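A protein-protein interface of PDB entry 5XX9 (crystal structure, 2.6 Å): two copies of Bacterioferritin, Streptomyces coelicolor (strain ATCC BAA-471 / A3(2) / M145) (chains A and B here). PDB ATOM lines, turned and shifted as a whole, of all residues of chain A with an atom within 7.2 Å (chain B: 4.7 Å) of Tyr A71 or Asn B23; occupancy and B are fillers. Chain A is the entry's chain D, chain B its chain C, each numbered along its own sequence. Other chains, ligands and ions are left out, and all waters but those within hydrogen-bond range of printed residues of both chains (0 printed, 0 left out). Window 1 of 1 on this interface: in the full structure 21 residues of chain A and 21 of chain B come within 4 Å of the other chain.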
ATOM      1  N   ASN A  12       7.103  23.034 -26.731  1.00  0.00           N
ATOM      2  CA  ASN A  12       8.265  22.419 -27.347  1.00  0.00           C
ATOM      3  C   ASN A  12       8.681  23.160 -28.608  1.00  0.00           C
ATOM      4  O   ASN A  12       9.871  23.195 -28.946  1.00  0.00           O
ATOM      5  CB  ASN A  12       7.978  20.944 -27.644  1.00  0.00           C
ATOM      6  CG  ASN A  12       8.585  20.022 -26.615  1.00  0.00           C
ATOM      7  OD1 ASN A  12       9.611  20.348 -26.009  1.00  0.00           O
ATOM      8  ND2 ASN A  12       7.969  18.861 -26.410  1.00  0.00           N
ATOM      9  N   LEU A  15      10.494  26.119 -27.400  1.00  0.00           N
ATOM     10  CA  LEU A  15      11.746  25.611 -26.852  1.00  0.00           C
ATOM     11  C   LEU A  15      12.768  25.385 -27.954  1.00  0.00           C
ATOM     12  O   LEU A  15      13.944  25.746 -27.808  1.00  0.00           O
ATOM     13  CB  LEU A  15      11.493  24.312 -26.080  1.00  0.00           C
ATOM     14  CG  LEU A  15      12.781  23.639 -25.584  1.00  0.00           C
ATOM     15  CD1 LEU A  15      13.614  24.586 -24.708  1.00  0.00           C
ATOM     16  CD2 LEU A  15      12.490  22.323 -24.845  1.00  0.00           C
ATOM     17  N   THR A  16      12.335  24.782 -29.068  1.00  0.00           N
ATOM     18  CA  THR A  16      13.218  24.633 -30.220  1.00  0.00           C
ATOM     19  C   THR A  16      13.731  25.992 -30.681  1.00  0.00           C
ATOM     20  O   THR A  16      14.921  26.155 -30.964  1.00  0.00           O
ATOM     21  CB  THR A  16      12.485  23.923 -31.371  1.00  0.00           C
ATOM     22  OG1 THR A  16      12.126  22.589 -31.000  1.00  0.00           O
ATOM     23  CG2 THR A  16      13.362  23.864 -32.630  1.00  0.00           C
ATOM     24  N   LEU A  19      16.451  27.231 -28.173  1.00  0.00           N
ATOM     25  CA  LEU A  19      17.718  26.540 -28.376  1.00  0.00           C
ATOM     26  C   LEU A  19      18.393  27.036 -29.645  1.00  0.00           C
ATOM     27  O   LEU A  19      19.618  27.211 -29.676  1.00  0.00           O
ATOM     28  CB  LEU A  19      17.506  25.024 -28.428  1.00  0.00           C
ATOM     29  CG  LEU A  19      16.970  24.389 -27.145  1.00  0.00           C
ATOM     30  CD1 LEU A  19      16.696  22.925 -27.362  1.00  0.00           C
ATOM     31  CD2 LEU A  19      17.967  24.564 -26.009  1.00  0.00           C
ATOM     32  N   ILE A  22      19.719  30.478 -28.829  1.00  0.00           N
ATOM     33  CA  ILE A  22      20.915  30.389 -27.996  1.00  0.00           C
ATOM     34  C   ILE A  22      22.149  30.201 -28.866  1.00  0.00           C
ATOM     35  O   ILE A  22      23.143  30.926 -28.726  1.00  0.00           O
ATOM     36  CB  ILE A  22      20.775  29.256 -26.966  1.00  0.00           C
ATOM     37  CG1 ILE A  22      19.637  29.567 -25.998  1.00  0.00           C
ATOM     38  CG2 ILE A  22      22.104  29.042 -26.204  1.00  0.00           C
ATOM     39  CD1 ILE A  22      19.116  28.319 -25.276  1.00  0.00           C
ATOM     40  N   ASN A  23      22.100  29.230 -29.782  1.00  0.00           N
ATOM     41  CA  ASN A  23      23.244  28.982 -30.648  1.00  0.00           C
ATOM     42  C   ASN A  23      23.523  30.185 -31.533  1.00  0.00           C
ATOM     43  O   ASN A  23      24.670  30.627 -31.651  1.00  0.00           O
ATOM     44  CB  ASN A  23      23.008  27.722 -31.482  1.00  0.00           C
ATOM     45  CG  ASN A  23      23.190  26.446 -30.668  1.00  0.00           C
ATOM     46  OD1 ASN A  23      23.286  26.501 -29.449  1.00  0.00           O
ATOM     47  ND2 ASN A  23      23.223  25.301 -31.333  1.00  0.00           N
ATOM     48  N   MET A  52      18.722  31.326 -22.816  1.00  0.00           N
ATOM     49  CA  MET A  52      18.871  30.123 -21.999  1.00  0.00           C
ATOM     50  C   MET A  52      17.867  30.100 -20.862  1.00  0.00           C
ATOM     51  O   MET A  52      17.290  29.051 -20.547  1.00  0.00           O
ATOM     52  CB  MET A  52      20.285  30.021 -21.446  1.00  0.00           C
ATOM     53  CG  MET A  52      21.323  29.710 -22.468  1.00  0.00           C
ATOM     54  SD  MET A  52      22.949  29.702 -21.715  1.00  0.00           S
ATOM     55  CE  MET A  52      23.972  29.976 -23.155  1.00  0.00           C
ATOM     56  N   ALA A  55      14.679  28.960 -22.287  1.00  0.00           N
ATOM     57  CA  ALA A  55      14.717  27.512 -22.454  1.00  0.00           C
ATOM     58  C   ALA A  55      14.462  26.786 -21.136  1.00  0.00           C
ATOM     59  O   ALA A  55      13.685  25.821 -21.094  1.00  0.00           O
ATOM     60  CB  ALA A  55      16.058  27.087 -23.054  1.00  0.00           C
ATOM     61  N   GLU A  56      15.092  27.240 -20.046  1.00  0.00           N
ATOM     62  CA  GLU A  56      14.906  26.537 -18.781  1.00  0.00           C
ATOM     63  C   GLU A  56      13.483  26.699 -18.265  1.00  0.00           C
ATOM     64  O   GLU A  56      12.887  25.735 -17.773  1.00  0.00           O
ATOM     65  CB  GLU A  56      15.910  27.007 -17.724  1.00  0.00           C
ATOM     66  CG  GLU A  56      15.740  26.253 -16.410  1.00  0.00           C
ATOM     67  CD  GLU A  56      16.994  26.195 -15.563  1.00  0.00           C
ATOM     68  OE1 GLU A  56      17.810  27.145 -15.658  1.00  0.00           O
ATOM     69  OE2 GLU A  56      17.150  25.197 -14.813  1.00  0.00           O
ATOM     70  N   VAL A  57      12.905  27.893 -18.407  1.00  0.00           N
ATOM     71  CA  VAL A  57      11.527  28.091 -17.970  1.00  0.00           C
ATOM     72  C   VAL A  57      10.592  27.190 -18.767  1.00  0.00           C
ATOM     73  O   VAL A  57       9.686  26.559 -18.207  1.00  0.00           O
ATOM     74  CB  VAL A  57      11.124  29.579 -18.077  1.00  0.00           C
ATOM     75  CG1 VAL A  57       9.622  29.748 -17.902  1.00  0.00           C
ATOM     76  CG2 VAL A  57      11.874  30.420 -17.058  1.00  0.00           C
ATOM     77  N   LEU A  58      10.787  27.111 -20.086  1.00  0.00           N
ATOM     78  CA  LEU A  58       9.955  26.221 -20.887  1.00  0.00           C
ATOM     79  C   LEU A  58      10.132  24.764 -20.467  1.00  0.00           C
ATOM     80  O   LEU A  58       9.149  24.046 -20.243  1.00  0.00           O
ATOM     81  CB  LEU A  58      10.283  26.396 -22.366  1.00  0.00           C
ATOM     82  CG  LEU A  58       9.779  27.703 -22.961  1.00  0.00           C
ATOM     83  CD1 LEU A  58      10.421  27.942 -24.333  1.00  0.00           C
ATOM     84  CD2 LEU A  58       8.245  27.652 -23.055  1.00  0.00           C
ATOM     85  N   THR A  59      11.386  24.324 -20.316  1.00  0.00           N
ATOM     86  CA  THR A  59      11.639  22.944 -19.908  1.00  0.00           C
ATOM     87  C   THR A  59      10.937  22.614 -18.595  1.00  0.00           C
ATOM     88  O   THR A  59      10.331  21.546 -18.469  1.00  0.00           O
ATOM     89  CB  THR A  59      13.148  22.685 -19.816  1.00  0.00           C
ATOM     90  OG1 THR A  59      13.740  22.821 -21.113  1.00  0.00           O
ATOM     91  CG2 THR A  59      13.443  21.308 -19.274  1.00  0.00           C
ATOM     92  N   ASP A  60      10.993  23.522 -17.622  1.00  0.00           N
ATOM     93  CA  ASP A  60      10.353  23.267 -16.334  1.00  0.00           C
ATOM     94  C   ASP A  60       8.868  23.008 -16.509  1.00  0.00           C
ATOM     95  O   ASP A  60       8.313  22.076 -15.911  1.00  0.00           O
ATOM     96  CB  ASP A  60      10.557  24.446 -15.390  1.00  0.00           C
ATOM     97  CG  ASP A  60      11.854  24.368 -14.621  1.00  0.00           C
ATOM     98  OD1 ASP A  60      12.515  23.313 -14.657  1.00  0.00           O
ATOM     99  OD2 ASP A  60      12.192  25.358 -13.946  1.00  0.00           O
ATOM    100  N   ILE A  62       7.208  22.130 -19.295  1.00  0.00           N
ATOM    101  CA  ILE A  62       6.964  20.904 -20.043  1.00  0.00           C
ATOM    102  C   ILE A  62       7.035  19.706 -19.107  1.00  0.00           C
ATOM    103  O   ILE A  62       6.174  18.825 -19.140  1.00  0.00           O
ATOM    104  CB  ILE A  62       7.953  20.782 -21.210  1.00  0.00           C
ATOM    105  CG1 ILE A  62       7.672  21.880 -22.236  1.00  0.00           C
ATOM    106  CG2 ILE A  62       7.878  19.411 -21.857  1.00  0.00           C
ATOM    107  CD1 ILE A  62       8.757  22.105 -23.216  1.00  0.00           C
ATOM    108  N   LEU A  68       7.842  15.509 -22.790  1.00  0.00           N
ATOM    109  CA  LEU A  68       9.279  15.314 -22.958  1.00  0.00           C
ATOM    110  C   LEU A  68       9.875  16.550 -23.623  1.00  0.00           C
ATOM    111  O   LEU A  68       9.566  16.817 -24.793  1.00  0.00           O
ATOM    112  CB  LEU A  68       9.585  14.052 -23.778  1.00  0.00           C
ATOM    113  CG  LEU A  68      11.067  13.638 -23.987  1.00  0.00           C
ATOM    114  CD1 LEU A  68      11.749  14.248 -25.221  1.00  0.00           C
ATOM    115  CD2 LEU A  68      11.936  13.916 -22.752  1.00  0.00           C
ATOM    116  N   PRO A  69      10.686  17.338 -22.925  1.00  0.00           N
ATOM    117  CA  PRO A  69      11.308  18.507 -23.569  1.00  0.00           C
ATOM    118  C   PRO A  69      12.168  18.073 -24.749  1.00  0.00           C
ATOM    119  O   PRO A  69      12.924  17.106 -24.662  1.00  0.00           O
ATOM    120  CB  PRO A  69      12.156  19.127 -22.446  1.00  0.00           C
ATOM    121  CG  PRO A  69      11.628  18.551 -21.169  1.00  0.00           C
ATOM    122  CD  PRO A  69      11.088  17.189 -21.518  1.00  0.00           C
ATOM    123  N   ASN A  70      12.020  18.773 -25.869  1.00  0.00           N
ATOM    124  CA  ASN A  70      12.744  18.432 -27.095  1.00  0.00           C
ATOM    125  C   ASN A  70      14.088  19.154 -27.083  1.00  0.00           C
ATOM    126  O   ASN A  70      14.159  20.361 -27.322  1.00  0.00           O
ATOM    127  CB  ASN A  70      11.928  18.808 -28.326  1.00  0.00           C
ATOM    128  CG  ASN A  70      12.499  18.213 -29.613  1.00  0.00           C
ATOM    129  OD1 ASN A  70      13.698  17.911 -29.699  1.00  0.00           O
ATOM    130  ND2 ASN A  70      11.640  18.046 -30.625  1.00  0.00           N
ATOM    131  N   TYR A  71      15.160  18.420 -26.792  1.00  0.00           N
ATOM    132  CA  TYR A  71      16.511  18.964 -26.889  1.00  0.00           C
ATOM    133  C   TYR A  71      17.274  18.410 -28.091  1.00  0.00           C
ATOM    134  O   TYR A  71      18.499  18.523 -28.139  1.00  0.00           O
ATOM    135  CB  TYR A  71      17.292  18.714 -25.592  1.00  0.00           C
ATOM    136  CG  TYR A  71      17.053  19.770 -24.529  1.00  0.00           C
ATOM    137  CD1 TYR A  71      15.841  19.829 -23.832  1.00  0.00           C
ATOM    138  CD2 TYR A  71      18.040  20.712 -24.222  1.00  0.00           C
ATOM    139  CE1 TYR A  71      15.624  20.809 -22.865  1.00  0.00           C
ATOM    140  CE2 TYR A  71      17.835  21.679 -23.251  1.00  0.00           C
ATOM    141  CZ  TYR A  71      16.623  21.732 -22.585  1.00  0.00           C
ATOM    142  OH  TYR A  71      16.402  22.699 -21.630  1.00  0.00           O
ATOM    143  N   GLN A  72      16.570  17.830 -29.063  1.00  0.00           N
ATOM    144  CA  GLN A  72      17.181  17.252 -30.251  1.00  0.00           C
ATOM    145  C   GLN A  72      17.055  18.143 -31.483  1.00  0.00           C
ATOM    146  O   GLN A  72      17.966  18.167 -32.324  1.00  0.00           O
ATOM    147  CB  GLN A  72      16.553  15.886 -30.554  1.00  0.00           C
ATOM    148  CG  GLN A  72      17.199  15.097 -31.714  1.00  0.00           C
ATOM    149  CD  GLN A  72      18.652  14.732 -31.465  1.00  0.00           C
ATOM    150  OE1 GLN A  72      18.949  13.773 -30.743  1.00  0.00           O
ATOM    151  NE2 GLN A  72      19.567  15.497 -32.054  1.00  0.00           N
ATOM    152  N   ARG A  73      15.980  18.917 -31.590  1.00  0.00           N
ATOM    153  CA  ARG A  73      15.649  19.589 -32.835  1.00  0.00           C
ATOM    154  C   ARG A  73      16.186  21.014 -32.818  1.00  0.00           C
ATOM    155  O   ARG A  73      16.265  21.648 -31.762  1.00  0.00           O
ATOM    156  CB  ARG A  73      14.128  19.567 -33.032  1.00  0.00           C
ATOM    157  CG  ARG A  73      13.553  20.416 -34.155  1.00  0.00           C
ATOM    158  CD  ARG A  73      12.026  20.257 -34.202  1.00  0.00           C
ATOM    159  NE  ARG A  73      11.380  20.916 -33.064  1.00  0.00           N
ATOM    160  CZ  ARG A  73      10.136  20.682 -32.658  1.00  0.00           C
ATOM    161  NH1 ARG A  73       9.378  19.798 -33.293  1.00  0.00           N
ATOM    162  NH2 ARG A  73       9.660  21.315 -31.592  1.00  0.00           N
ATOM    163  N   LEU A  74      16.641  21.479 -33.980  1.00  0.00           N
ATOM    164  CA  LEU A  74      16.989  22.877 -34.169  1.00  0.00           C
ATOM    165  C   LEU A  74      16.399  23.389 -35.470  1.00  0.00           C
ATOM    166  O   LEU A  74      16.331  22.669 -36.469  1.00  0.00           O
ATOM    167  CB  LEU A  74      18.503  23.127 -34.194  1.00  0.00           C
ATOM    168  CG  LEU A  74      19.277  23.066 -32.884  1.00  0.00           C
ATOM    169  CD1 LEU A  74      20.781  23.104 -33.144  1.00  0.00           C
ATOM    170  CD2 LEU A  74      18.843  24.189 -31.979  1.00  0.00           C
ATOM    171  N   LEU B  19      28.179  20.231 -28.072  1.00  0.00           N
ATOM    172  CA  LEU B  19      26.816  20.750 -28.129  1.00  0.00           C
ATOM    173  C   LEU B  19      25.808  19.645 -27.858  1.00  0.00           C
ATOM    174  O   LEU B  19      24.819  19.862 -27.150  1.00  0.00           O
ATOM    175  CB  LEU B  19      26.532  21.416 -29.475  1.00  0.00           C
ATOM    176  CG  LEU B  19      27.358  22.660 -29.780  1.00  0.00           C
ATOM    177  CD1 LEU B  19      27.045  23.237 -31.175  1.00  0.00           C
ATOM    178  CD2 LEU B  19      27.123  23.676 -28.685  1.00  0.00           C
ATOM    179  N   THR B  20      26.063  18.443 -28.380  1.00  0.00           N
ATOM    180  CA  THR B  20      25.197  17.315 -28.065  1.00  0.00           C
ATOM    181  C   THR B  20      25.212  17.044 -26.563  1.00  0.00           C
ATOM    182  O   THR B  20      24.158  16.935 -25.924  1.00  0.00           O
ATOM    183  CB  THR B  20      25.657  16.077 -28.855  1.00  0.00           C
ATOM    184  OG1 THR B  20      25.798  16.405 -30.243  1.00  0.00           O
ATOM    185  CG2 THR B  20      24.687  14.901 -28.711  1.00  0.00           C
ATOM    186  N   ALA B  21      26.411  17.002 -25.974  1.00  0.00           N
ATOM    187  CA  ALA B  21      26.541  16.699 -24.549  1.00  0.00           C
ATOM    188  C   ALA B  21      25.891  17.760 -23.668  1.00  0.00           C
ATOM    189  O   ALA B  21      25.342  17.435 -22.610  1.00  0.00           O
ATOM    190  CB  ALA B  21      28.015  16.528 -24.180  1.00  0.00           C
ATOM    191  N   ILE B  22      25.999  19.041 -24.040  1.00  0.00           N
ATOM    192  CA  ILE B  22      25.353  20.073 -23.236  1.00  0.00           C
ATOM    193  C   ILE B  22      23.862  19.800 -23.160  1.00  0.00           C
ATOM    194  O   ILE B  22      23.269  19.776 -22.081  1.00  0.00           O
ATOM    195  CB  ILE B  22      25.630  21.474 -23.802  1.00  0.00           C
ATOM    196  CG1 ILE B  22      27.113  21.814 -23.749  1.00  0.00           C
ATOM    197  CG2 ILE B  22      24.880  22.511 -22.997  1.00  0.00           C
ATOM    198  CD1 ILE B  22      27.494  22.966 -24.687  1.00  0.00           C
ATOM    199  N   ASN B  23      23.233  19.578 -24.310  1.00  0.00           N
ATOM    200  CA  ASN B  23      21.803  19.318 -24.308  1.00  0.00           C
ATOM    201  C   ASN B  23      21.492  18.043 -23.540  1.00  0.00           C
ATOM    202  O   ASN B  23      20.571  18.017 -22.713  1.00  0.00           O
ATOM    203  CB  ASN B  23      21.276  19.237 -25.740  1.00  0.00           C
ATOM    204  CG  ASN B  23      21.136  20.606 -26.384  1.00  0.00           C
ATOM    205  OD1 ASN B  23      21.635  21.594 -25.866  1.00  0.00           O
ATOM    206  ND2 ASN B  23      20.435  20.671 -27.502  1.00  0.00           N
ATOM    207  N   GLN B  24      22.282  16.984 -23.770  1.00  0.00           N
ATOM    208  CA  GLN B  24      21.998  15.706 -23.125  1.00  0.00           C
ATOM    209  C   GLN B  24      22.138  15.817 -21.611  1.00  0.00           C
ATOM    210  O   GLN B  24      21.296  15.314 -20.849  1.00  0.00           O
ATOM    211  CB  GLN B  24      22.910  14.608 -23.669  1.00  0.00           C
ATOM    212  CG  GLN B  24      22.577  13.234 -23.053  1.00  0.00           C
ATOM    213  CD  GLN B  24      23.225  12.067 -23.788  1.00  0.00           C
ATOM    214  OE1 GLN B  24      23.082  11.927 -25.007  1.00  0.00           O
ATOM    215  NE2 GLN B  24      23.918  11.206 -23.039  1.00  0.00           N
ATOM    216  N   TYR B  25      23.212  16.459 -21.157  1.00  0.00           N
ATOM    217  CA  TYR B  25      23.432  16.566 -19.725  1.00  0.00           C
ATOM    218  C   TYR B  25      22.430  17.513 -19.093  1.00  0.00           C
ATOM    219  O   TYR B  25      21.917  17.243 -18.002  1.00  0.00           O
ATOM    220  CB  TYR B  25      24.849  17.041 -19.437  1.00  0.00           C
ATOM    221  CG  TYR B  25      25.916  16.086 -19.872  1.00  0.00           C
ATOM    222  CD1 TYR B  25      25.603  14.813 -20.348  1.00  0.00           C
ATOM    223  CD2 TYR B  25      27.249  16.447 -19.793  1.00  0.00           C
ATOM    224  CE1 TYR B  25      26.606  13.936 -20.737  1.00  0.00           C
ATOM    225  CE2 TYR B  25      28.244  15.586 -20.178  1.00  0.00           C
ATOM    226  CZ  TYR B  25      27.933  14.337 -20.647  1.00  0.00           C
ATOM    227  OH  TYR B  25      28.967  13.508 -21.030  1.00  0.00           O
ATOM    228  N   PHE B  26      22.126  18.619 -19.772  1.00  0.00           N
ATOM    229  CA  PHE B  26      21.194  19.570 -19.198  1.00  0.00           C
ATOM    230  C   PHE B  26      19.822  18.943 -19.042  1.00  0.00           C
ATOM    231  O   PHE B  26      19.187  19.078 -17.991  1.00  0.00           O
ATOM    232  CB  PHE B  26      21.108  20.832 -20.051  1.00  0.00           C
ATOM    233  CG  PHE B  26      20.371  21.949 -19.376  1.00  0.00           C
ATOM    234  CD1 PHE B  26      20.997  22.702 -18.385  1.00  0.00           C
ATOM    235  CD2 PHE B  26      19.046  22.209 -19.683  1.00  0.00           C
ATOM    236  CE1 PHE B  26      20.324  23.714 -17.729  1.00  0.00           C
ATOM    237  CE2 PHE B  26      18.360  23.213 -19.024  1.00  0.00           C
ATOM    238  CZ  PHE B  26      19.001  23.981 -18.044  1.00  0.00           C
ATOM    239  N   LEU B  27      19.360  18.227 -20.064  1.00  0.00           N
ATOM    240  CA  LEU B  27      18.051  17.591 -19.976  1.00  0.00           C
ATOM    241  C   LEU B  27      18.038  16.509 -18.901  1.00  0.00           C
ATOM    242  O   LEU B  27      17.061  16.378 -18.157  1.00  0.00           O
ATOM    243  CB  LEU B  27      17.648  17.033 -21.340  1.00  0.00           C
ATOM    244  CG  LEU B  27      16.341  16.252 -21.322  1.00  0.00           C
ATOM    245  CD1 LEU B  27      15.206  17.165 -20.887  1.00  0.00           C
ATOM    246  CD2 LEU B  27      16.057  15.655 -22.681  1.00  0.00           C
ATOM    247  N   LEU B  74      23.699  18.574 -34.625  1.00  0.00           N
ATOM    248  CA  LEU B  74      23.745  17.824 -33.380  1.00  0.00           C
ATOM    249  C   LEU B  74      23.803  16.334 -33.669  1.00  0.00           C
ATOM    250  O   LEU B  74      23.222  15.858 -34.649  1.00  0.00           O
ATOM    251  CB  LEU B  74      22.546  18.114 -32.484  1.00  0.00           C
ATOM    252  CG  LEU B  74      22.599  19.483 -31.817  1.00  0.00           C
ATOM    253  CD1 LEU B  74      21.263  19.829 -31.152  1.00  0.00           C
ATOM    254  CD2 LEU B  74      23.762  19.531 -30.844  1.00  0.00           C
ATOM    255  N   VAL B  77      20.772  12.889 -29.324  1.00  0.00           N
ATOM    256  CA  VAL B  77      20.703  13.099 -27.886  1.00  0.00           C
ATOM    257  C   VAL B  77      20.070  11.861 -27.255  1.00  0.00           C
ATOM    258  O   VAL B  77      18.967  11.469 -27.623  1.00  0.00           O
ATOM    259  CB  VAL B  77      19.902  14.370 -27.564  1.00  0.00           C
ATOM    260  CG1 VAL B  77      19.649  14.508 -26.053  1.00  0.00           C
ATOM    261  CG2 VAL B  77      20.638  15.593 -28.104  1.00  0.00           C
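ND2 of Asn B23 sits at hydrogen-bond distance from O of Tyr A71 (3.0 Å). The backbone NH (N) of Val B77 is in hydrogen-bond range of the side-chain amide oxygen (OE1) of Gln A72 (2.5 Å).
The side-chain hydroxyl (OH) of Tyr A71 sits at hydrogen-bond distance from the side-chain hydroxyl (OG1) of Thr A59 (2.7 Å). The backbone NH (N) of Gln A72 is in hydrogen-bond range of the side-chain amide oxygen (OD1) of Asn A70 (2.9 Å).
Among the printed residues, merely in contact across the chains: Tyr A71 with Phe B26 (3.3 Å), Tyr A71 with Val B77 (3.6 Å), Pro A69 with Leu B27 (3.8 Å), Leu A74 with Leu B74 (3.9 Å), Gln A72 with Leu B74 (3.9 Å) and Glu A56 with Phe B26 (3.9 Å).
Of the printed residues of chain B, Glu A56 touches Phe B26 (3.9 Å). Of the printed residues of chain B, Gln A72 touches Leu B74 and Val B77. Of chain A, only Tyr A71 (3.0 Å) comes within 4 Å of Asn B23. Printed residues of chain A within 4 Å of Leu B27: Pro A69. The nearest residue of chain B that does not touch Tyr A71 is Leu B27 (4.02 Å). The nearest residue of chain A that does not touch Asn B23 is Leu A19 (4.4 Å).
Of the 11 printed residues of chain B, 5 touch a printed residue of chain A. Hydrophobic or aromatic side chains of chain B that line the printed part of chain A: Phe B26, Leu B27, Leu B74 and Val B77. Hydrophobic or aromatic side chains of chain A within 4 Å of the printed part of chain B: Pro A69, Tyr A71 and Leu A74.
Leu A74 touches its own counterpart, Leu B74. Of the 8 pairs that touch across the chains among the printed residues, 1 has its exchanged pair printed and touching as well.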
